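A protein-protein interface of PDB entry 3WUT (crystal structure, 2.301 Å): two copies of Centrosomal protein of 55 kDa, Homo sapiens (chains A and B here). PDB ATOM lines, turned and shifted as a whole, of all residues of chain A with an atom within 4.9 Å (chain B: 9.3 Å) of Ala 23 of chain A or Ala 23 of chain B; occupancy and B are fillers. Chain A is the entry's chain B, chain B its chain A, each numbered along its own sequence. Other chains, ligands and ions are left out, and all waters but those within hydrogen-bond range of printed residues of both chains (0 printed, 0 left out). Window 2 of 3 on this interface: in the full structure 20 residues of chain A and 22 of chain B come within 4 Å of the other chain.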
ATOM      1  N   GLN A  19      16.408 -18.751  21.524  1.00  0.00           N
ATOM      2  CA  GLN A  19      17.414 -19.687  22.000  1.00  0.00           C
ATOM      3  C   GLN A  19      16.900 -20.605  23.109  1.00  0.00           C
ATOM      4  O   GLN A  19      17.510 -21.638  23.380  1.00  0.00           O
ATOM      5  CB  GLN A  19      18.687 -18.958  22.432  1.00  0.00           C
ATOM      6  CG  GLN A  19      19.911 -19.330  21.598  1.00  0.00           C
ATOM      7  CD  GLN A  19      19.769 -18.944  20.134  1.00  0.00           C
ATOM      8  OE1 GLN A  19      19.137 -19.650  19.348  1.00  0.00           O
ATOM      9  NE2 GLN A  19      20.359 -17.813  19.764  1.00  0.00           N
ATOM     10  N   LEU A  20      15.785 -20.235  23.738  1.00  0.00           N
ATOM     11  CA  LEU A  20      15.111 -21.133  24.673  1.00  0.00           C
ATOM     12  C   LEU A  20      14.534 -22.294  23.901  1.00  0.00           C
ATOM     13  O   LEU A  20      14.537 -23.430  24.375  1.00  0.00           O
ATOM     14  CB  LEU A  20      13.982 -20.429  25.427  1.00  0.00           C
ATOM     15  CG  LEU A  20      13.183 -21.308  26.401  1.00  0.00           C
ATOM     16  CD1 LEU A  20      14.087 -22.046  27.385  1.00  0.00           C
ATOM     17  CD2 LEU A  20      12.148 -20.482  27.149  1.00  0.00           C
ATOM     18  N   LYS A  21      14.043 -22.011  22.700  1.00  0.00           N
ATOM     19  CA  LYS A  21      13.502 -23.066  21.861  1.00  0.00           C
ATOM     20  C   LYS A  21      14.613 -23.965  21.301  1.00  0.00           C
ATOM     21  O   LYS A  21      14.455 -25.186  21.261  1.00  0.00           O
ATOM     22  CB  LYS A  21      12.603 -22.495  20.763  1.00  0.00           C
ATOM     23  CG  LYS A  21      11.305 -21.916  21.309  1.00  0.00           C
ATOM     24  CD  LYS A  21      10.559 -21.144  20.247  1.00  0.00           C
ATOM     25  CE  LYS A  21       9.618 -20.137  20.875  1.00  0.00           C
ATOM     26  NZ  LYS A  21       9.269 -19.073  19.899  1.00  0.00           N
ATOM     27  N   ASP A  22      15.738 -23.375  20.901  1.00  0.00           N
ATOM     28  CA  ASP A  22      16.875 -24.164  20.420  1.00  0.00           C
ATOM     29  C   ASP A  22      17.498 -25.022  21.515  1.00  0.00           C
ATOM     30  O   ASP A  22      17.931 -26.147  21.264  1.00  0.00           O
ATOM     31  CB  ASP A  22      17.931 -23.261  19.801  1.00  0.00           C
ATOM     32  CG  ASP A  22      17.509 -22.742  18.459  1.00  0.00           C
ATOM     33  OD1 ASP A  22      16.956 -23.542  17.677  1.00  0.00           O
ATOM     34  OD2 ASP A  22      17.699 -21.535  18.191  1.00  0.00           O
ATOM     35  N   ALA A  23      17.550 -24.477  22.726  1.00  0.00           N
ATOM     36  CA  ALA A  23      18.017 -25.230  23.875  1.00  0.00           C
ATOM     37  C   ALA A  23      17.119 -26.448  24.058  1.00  0.00           C
ATOM     38  O   ALA A  23      17.610 -27.566  24.222  1.00  0.00           O
ATOM     39  CB  ALA A  23      18.030 -24.355  25.140  1.00  0.00           C
ATOM     40  N   LEU A  24      15.806 -26.232  23.997  1.00  0.00           N
ATOM     41  CA  LEU A  24      14.845 -27.312  24.182  1.00  0.00           C
ATOM     42  C   LEU A  24      14.840 -28.299  23.017  1.00  0.00           C
ATOM     43  O   LEU A  24      14.490 -29.465  23.192  1.00  0.00           O
ATOM     44  CB  LEU A  24      13.438 -26.756  24.416  1.00  0.00           C
ATOM     45  CG  LEU A  24      13.199 -26.136  25.794  1.00  0.00           C
ATOM     46  CD1 LEU A  24      11.892 -25.355  25.818  1.00  0.00           C
ATOM     47  CD2 LEU A  24      13.212 -27.202  26.879  1.00  0.00           C
ATOM     48  N   GLU A  25      15.241 -27.828  21.840  1.00  0.00           N
ATOM     49  CA  GLU A  25      15.333 -28.681  20.669  1.00  0.00           C
ATOM     50  C   GLU A  25      16.477 -29.676  20.811  1.00  0.00           C
ATOM     51  O   GLU A  25      16.299 -30.882  20.615  1.00  0.00           O
ATOM     52  CB  GLU A  25      15.559 -27.853  19.411  1.00  0.00           C
ATOM     53  CG  GLU A  25      15.429 -28.686  18.148  1.00  0.00           C
ATOM     54  CD  GLU A  25      16.030 -28.034  16.931  1.00  0.00           C
ATOM     55  OE1 GLU A  25      15.904 -28.616  15.838  1.00  0.00           O
ATOM     56  OE2 GLU A  25      16.637 -26.953  17.063  1.00  0.00           O
ATOM     57  N   LYS A  26      17.658 -29.156  21.137  1.00  0.00           N
ATOM     58  CA  LYS A  26      18.829 -29.993  21.334  1.00  0.00           C
ATOM     59  C   LYS A  26      18.534 -30.906  22.489  1.00  0.00           C
ATOM     60  O   LYS A  26      18.780 -32.111  22.418  1.00  0.00           O
ATOM     61  CB  LYS A  26      20.047 -29.143  21.645  1.00  0.00           C
ATOM     62  CG  LYS A  26      20.989 -29.032  20.468  1.00  0.00           C
ATOM     63  CD  LYS A  26      21.176 -27.599  20.030  1.00  0.00           C
ATOM     64  CE  LYS A  26      22.154 -27.535  18.870  1.00  0.00           C
ATOM     65  NZ  LYS A  26      22.179 -26.193  18.228  1.00  0.00           N
ATOM     66  N   ASN A  27      17.975 -30.328  23.545  1.00  0.00           N
ATOM     67  CA  ASN A  27      17.560 -31.132  24.684  1.00  0.00           C
ATOM     68  C   ASN A  27      16.701 -32.327  24.254  1.00  0.00           C
ATOM     69  O   ASN A  27      16.823 -33.415  24.809  1.00  0.00           O
ATOM     70  CB  ASN A  27      16.866 -30.296  25.765  1.00  0.00           C
ATOM     71  CG  ASN A  27      16.698 -31.058  27.080  1.00  0.00           C
ATOM     72  OD1 ASN A  27      15.577 -31.323  27.527  1.00  0.00           O
ATOM     73  ND2 ASN A  27      17.814 -31.418  27.700  1.00  0.00           N
ATOM     74  N   GLU B  15      10.490 -16.343  35.051  1.00  0.00           N
ATOM     75  CA  GLU B  15      10.248 -17.762  34.783  1.00  0.00           C
ATOM     76  C   GLU B  15      10.884 -18.225  33.469  1.00  0.00           C
ATOM     77  O   GLU B  15      11.493 -19.297  33.409  1.00  0.00           O
ATOM     78  CB  GLU B  15       8.742 -18.057  34.772  1.00  0.00           C
ATOM     79  CG  GLU B  15       8.374 -19.404  34.156  1.00  0.00           C
ATOM     80  CD  GLU B  15       7.100 -19.357  33.311  1.00  0.00           C
ATOM     81  OE1 GLU B  15       6.669 -18.245  32.928  1.00  0.00           O
ATOM     82  OE2 GLU B  15       6.534 -20.437  33.023  1.00  0.00           O
ATOM     83  N   MET B  16      10.751 -17.413  32.424  1.00  0.00           N
ATOM     84  CA  MET B  16      11.340 -17.731  31.129  1.00  0.00           C
ATOM     85  C   MET B  16      12.874 -17.704  31.168  1.00  0.00           C
ATOM     86  O   MET B  16      13.535 -18.477  30.472  1.00  0.00           O
ATOM     87  CB  MET B  16      10.825 -16.771  30.060  1.00  0.00           C
ATOM     88  CG  MET B  16      11.230 -17.149  28.658  1.00  0.00           C
ATOM     89  SD  MET B  16      10.817 -15.878  27.458  1.00  0.00           S
ATOM     90  CE  MET B  16      11.447 -14.403  28.267  1.00  0.00           C
ATOM     91  N   GLU B  17      13.434 -16.811  31.979  1.00  0.00           N
ATOM     92  CA  GLU B  17      14.875 -16.759  32.162  1.00  0.00           C
ATOM     93  C   GLU B  17      15.338 -17.954  32.970  1.00  0.00           C
ATOM     94  O   GLU B  17      16.386 -18.524  32.683  1.00  0.00           O
ATOM     95  CB  GLU B  17      15.288 -15.479  32.878  1.00  0.00           C
ATOM     96  CG  GLU B  17      15.175 -14.234  32.023  1.00  0.00           C
ATOM     97  CD  GLU B  17      15.147 -12.962  32.853  1.00  0.00           C
ATOM     98  OE1 GLU B  17      15.867 -12.892  33.878  1.00  0.00           O
ATOM     99  OE2 GLU B  17      14.393 -12.039  32.479  1.00  0.00           O
ATOM    100  N   ILE B  18      14.553 -18.316  33.987  1.00  0.00           N
ATOM    101  CA  ILE B  18      14.817 -19.499  34.807  1.00  0.00           C
ATOM    102  C   ILE B  18      14.962 -20.725  33.928  1.00  0.00           C
ATOM    103  O   ILE B  18      15.924 -21.482  34.057  1.00  0.00           O
ATOM    104  CB  ILE B  18      13.683 -19.767  35.835  1.00  0.00           C
ATOM    105  CG1 ILE B  18      13.654 -18.672  36.907  1.00  0.00           C
ATOM    106  CG2 ILE B  18      13.825 -21.164  36.458  1.00  0.00           C
ATOM    107  CD1 ILE B  18      15.018 -18.296  37.450  1.00  0.00           C
ATOM    108  N   GLN B  19      14.004 -20.899  33.021  1.00  0.00           N
ATOM    109  CA  GLN B  19      13.962 -22.066  32.153  1.00  0.00           C
ATOM    110  C   GLN B  19      15.176 -22.163  31.231  1.00  0.00           C
ATOM    111  O   GLN B  19      15.742 -23.246  31.057  1.00  0.00           O
ATOM    112  CB  GLN B  19      12.680 -22.070  31.328  1.00  0.00           C
ATOM    113  CG  GLN B  19      11.423 -22.328  32.133  1.00  0.00           C
ATOM    114  CD  GLN B  19      10.243 -22.631  31.243  1.00  0.00           C
ATOM    115  OE1 GLN B  19      10.393 -23.261  30.196  1.00  0.00           O
ATOM    116  NE2 GLN B  19       9.060 -22.179  31.648  1.00  0.00           N
ATOM    117  N   LEU B  20      15.584 -21.041  30.646  1.00  0.00           N
ATOM    118  CA  LEU B  20      16.697 -21.079  29.712  1.00  0.00           C
ATOM    119  C   LEU B  20      18.007 -21.464  30.382  1.00  0.00           C
ATOM    120  O   LEU B  20      18.749 -22.286  29.858  1.00  0.00           O
ATOM    121  CB  LEU B  20      16.841 -19.766  28.964  1.00  0.00           C
ATOM    122  CG  LEU B  20      17.089 -19.980  27.472  1.00  0.00           C
ATOM    123  CD1 LEU B  20      16.736 -18.735  26.759  1.00  0.00           C
ATOM    124  CD2 LEU B  20      18.517 -20.316  27.165  1.00  0.00           C
ATOM    125  N   LYS B  21      18.279 -20.892  31.550  1.00  0.00           N
ATOM    126  CA  LYS B  21      19.494 -21.234  32.281  1.00  0.00           C
ATOM    127  C   LYS B  21      19.459 -22.670  32.802  1.00  0.00           C
ATOM    128  O   LYS B  21      20.505 -23.304  32.969  1.00  0.00           O
ATOM    129  CB  LYS B  21      19.748 -20.225  33.401  1.00  0.00           C
ATOM    130  CG  LYS B  21      20.317 -18.900  32.878  1.00  0.00           C
ATOM    131  CD  LYS B  21      20.321 -17.821  33.947  1.00  0.00           C
ATOM    132  CE  LYS B  21      19.025 -17.029  33.932  1.00  0.00           C
ATOM    133  NZ  LYS B  21      18.951 -16.084  35.064  1.00  0.00           N
ATOM    134  N   ASP B  22      18.247 -23.177  33.025  1.00  0.00           N
ATOM    135  CA  ASP B  22      18.031 -24.558  33.439  1.00  0.00           C
ATOM    136  C   ASP B  22      18.208 -25.500  32.254  1.00  0.00           C
ATOM    137  O   ASP B  22      18.789 -26.570  32.400  1.00  0.00           O
ATOM    138  CB  ASP B  22      16.638 -24.711  34.051  1.00  0.00           C
ATOM    139  CG  ASP B  22      16.333 -26.138  34.469  1.00  0.00           C
ATOM    140  OD1 ASP B  22      16.842 -26.575  35.524  1.00  0.00           O
ATOM    141  OD2 ASP B  22      15.567 -26.820  33.753  1.00  0.00           O
ATOM    142  N   ALA B  23      17.725 -25.084  31.085  1.00  0.00           N
ATOM    143  CA  ALA B  23      17.826 -25.887  29.865  1.00  0.00           C
ATOM    144  C   ALA B  23      19.254 -25.932  29.323  1.00  0.00           C
ATOM    145  O   ALA B  23      19.738 -26.985  28.899  1.00  0.00           O
ATOM    146  CB  ALA B  23      16.870 -25.358  28.799  1.00  0.00           C
ATOM    147  N   LEU B  24      19.922 -24.785  29.345  1.00  0.00           N
ATOM    148  CA  LEU B  24      21.287 -24.679  28.851  1.00  0.00           C
ATOM    149  C   LEU B  24      22.253 -25.575  29.602  1.00  0.00           C
ATOM    150  O   LEU B  24      23.027 -26.310  28.996  1.00  0.00           O
ATOM    151  CB  LEU B  24      21.767 -23.248  28.978  1.00  0.00           C
ATOM    152  CG  LEU B  24      21.303 -22.320  27.871  1.00  0.00           C
ATOM    153  CD1 LEU B  24      21.650 -20.923  28.310  1.00  0.00           C
ATOM    154  CD2 LEU B  24      21.975 -22.688  26.547  1.00  0.00           C
ATOM    155  N   GLU B  25      22.216 -25.501  30.925  1.00  0.00           N
ATOM    156  CA  GLU B  25      23.131 -26.290  31.725  1.00  0.00           C
ATOM    157  C   GLU B  25      22.656 -27.733  31.871  1.00  0.00           C
ATOM    158  O   GLU B  25      23.378 -28.575  32.405  1.00  0.00           O
ATOM    159  CB  GLU B  25      23.348 -25.646  33.089  1.00  0.00           C
ATOM    160  CG  GLU B  25      22.210 -25.826  34.062  1.00  0.00           C
ATOM    161  CD  GLU B  25      22.534 -25.227  35.410  1.00  0.00           C
ATOM    162  OE1 GLU B  25      23.330 -24.265  35.444  1.00  0.00           O
ATOM    163  OE2 GLU B  25      22.008 -25.721  36.432  1.00  0.00           O
ATOM    164  N   LYS B  26      21.448 -28.018  31.396  1.00  0.00           N
ATOM    165  CA  LYS B  26      20.974 -29.391  31.334  1.00  0.00           C
ATOM    166  C   LYS B  26      21.651 -30.123  30.176  1.00  0.00           C
ATOM    167  O   LYS B  26      22.037 -31.290  30.306  1.00  0.00           O
ATOM    168  CB  LYS B  26      19.454 -29.437  31.189  1.00  0.00           C
ATOM    169  CG  LYS B  26      18.736 -29.724  32.492  1.00  0.00           C
ATOM    170  CD  LYS B  26      17.250 -29.391  32.397  1.00  0.00           C
ATOM    171  CE  LYS B  26      16.468 -29.991  33.564  1.00  0.00           C
ATOM    172  NZ  LYS B  26      16.869 -29.450  34.890  1.00  0.00           N
ATOM    173  N   ASN B  27      21.792 -29.428  29.049  1.00  0.00           N
ATOM    174  CA  ASN B  27      22.481 -29.964  27.884  1.00  0.00           C
ATOM    175  C   ASN B  27      23.964 -30.129  28.167  1.00  0.00           C
ATOM    176  O   ASN B  27      24.623 -31.018  27.612  1.00  0.00           O
ATOM    177  CB  ASN B  27      22.302 -29.033  26.693  1.00  0.00           C
ATOM    178  CG  ASN B  27      20.904 -29.084  26.127  1.00  0.00           C
ATOM    179  OD1 ASN B  27      20.009 -29.705  26.703  1.00  0.00           O
ATOM    180  ND2 ASN B  27      20.705 -28.431  24.992  1.00  0.00           N
ATOM    181  N   GLN B  28      24.482 -29.251  29.025  1.00  0.00           N
ATOM    182  CA  GLN B  28      25.876 -29.295  29.431  1.00  0.00           C
ATOM    183  C   GLN B  28      26.070 -30.504  30.337  1.00  0.00           C
ATOM    184  O   GLN B  28      27.116 -31.147  30.309  1.00  0.00           O
ATOM    185  CB  GLN B  28      26.254 -28.004  30.161  1.00  0.00           C
ATOM    186  CG  GLN B  28      27.747 -27.708  30.192  1.00  0.00           C
ATOM    187  CD  GLN B  28      28.300 -27.302  28.839  1.00  0.00           C
ATOM    188  OE1 GLN B  28      27.579 -26.797  27.988  1.00  0.00           O
ATOM    189  NE2 GLN B  28      29.589 -27.521  28.641  1.00  0.00           N
ATOM    190  N   GLN B  29      25.041 -30.817  31.121  1.00  0.00           N
ATOM    191  CA  GLN B  29      25.038 -32.007  31.947  1.00  0.00           C
ATOM    192  C   GLN B  29      25.004 -33.258  31.080  1.00  0.00           C
ATOM    193  O   GLN B  29      25.610 -34.272  31.422  1.00  0.00           O
ATOM    194  CB  GLN B  29      23.832 -32.007  32.873  1.00  0.00           C
ATOM    195  CG  GLN B  29      23.955 -31.089  34.075  1.00  0.00           C
ATOM    196  CD  GLN B  29      22.653 -30.957  34.831  1.00  0.00           C
ATOM    197  OE1 GLN B  29      21.641 -31.568  34.475  1.00  0.00           O
ATOM    198  NE2 GLN B  29      22.669 -30.156  35.880  1.00  0.00           N
ATOM    199  N   TRP B  30      24.273 -33.184  29.972  1.00  0.00           N
ATOM    200  CA  TRP B  30      24.214 -34.279  29.017  1.00  0.00           C
ATOM    201  C   TRP B  30      25.579 -34.617  28.453  1.00  0.00           C
ATOM    202  O   TRP B  30      25.906 -35.788  28.295  1.00  0.00           O
ATOM    203  CB  TRP B  30      23.257 -33.954  27.871  1.00  0.00           C
ATOM    204  CG  TRP B  30      21.880 -34.369  28.193  1.00  0.00           C
ATOM    205  CD1 TRP B  30      20.794 -33.557  28.339  1.00  0.00           C
ATOM    206  CD2 TRP B  30      21.428 -35.703  28.467  1.00  0.00           C
ATOM    207  NE1 TRP B  30      19.691 -34.305  28.678  1.00  0.00           N
ATOM    208  CE2 TRP B  30      20.052 -35.623  28.756  1.00  0.00           C
ATOM    209  CE3 TRP B  30      22.048 -36.955  28.484  1.00  0.00           C
ATOM    210  CZ2 TRP B  30      19.289 -36.751  29.058  1.00  0.00           C
ATOM    211  CZ3 TRP B  30      21.284 -38.073  28.787  1.00  0.00           C
ATOM    212  CH2 TRP B  30      19.923 -37.962  29.071  1.00  0.00           C
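ND2 of Asn 27 of chain A lies within hydrogen-bond range of OD1 of Asn 27 of chain B, 3.0 Å away. The backbone carbonyl oxygen of Ala 23 of chain A sits at hydrogen-bond distance from the side-chain amide nitrogen of Asn 27 of chain B (3.3 Å).
The side-chain carboxylate (OE2) of Glu 15 of chain B sits at hydrogen-bond distance from the side-chain amide nitrogen (NE2) of Gln 19 of chain B (3.4 Å).
Among the printed residues, pairs that only touch across the chains: Lys 26 of chain A with Asn 27 of chain B (3.5 Å), Leu 20 of chain A with Leu 20 of chain B (3.5 Å), Asn 27 of chain A with Trp 30 of chain B (3.6 Å), Leu 20 of chain A with Met 16 of chain B (3.8 Å), Ala 23 of chain A with Ala 23 of chain B (3.97 Å) and Leu 20 of chain A with Gln 19 of chain B (3.999 Å).
Of the printed residues of chain B, Leu 20 of chain A touches Met 16 (3.8 Å), Gln 19 (3.999 Å) and Leu 20 (3.5 Å). Printed residues of chain B within 4 Å of Ala 23 of chain A: Ala 23 (3.97 Å) and Asn 27 (3.3 Å). Of the printed residues of chain A, Leu 20 of chain B touches Leu 20 (3.5 Å). Of chain A, only Ala 23 comes within 4 Å of Ala 23 of chain B. Lys 26 of chain B touches none of the printed residues of chain A. The nearest residue of chain B that does not touch Ala 23 of chain A is Leu 24 of chain B (4.5 Å). The nearest printed residue of chain A that does not touch Ala 23 of chain B is Leu 24 of chain A (4.5 Å). The nearest printed residue of chain A that does not touch Met 16 of chain B is Lys 21 of chain A (7.9 Å).
Of the 16 printed residues of chain B, 6 touch a printed residue of chain A. Printed residues of chain B that touch a printed residue of chain A: Met 16, Gln 19, Leu 20, Ala 23, Asn 27 and Trp 30. Hydrophobic or aromatic side chains of chain B that line the printed part of chain A: Met 16, Leu 20, Ala 23 and Trp 30. Among the printed residues, 8 pairs touch across the chains.
Leu 20 of chain A touches Gln 19 of chain B, but with the chains exchanged Gln 19 of chain A does not touch Leu 20 of chain B (4.1 Å). Ala 23 of chain B touches its own counterpart, Ala 23 of chain A. Ala 23 of chain A touches Asn 27 of chain B, but with the chains exchanged Asn 27 of chain A does not touch Ala 23 of chain B (5.0 Å). Lys 26 of chain A touches Asn 27 of chain B, but with the chains exchanged Asn 27 of chain A does not touch Lys 26 of chain B (4.3 Å).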
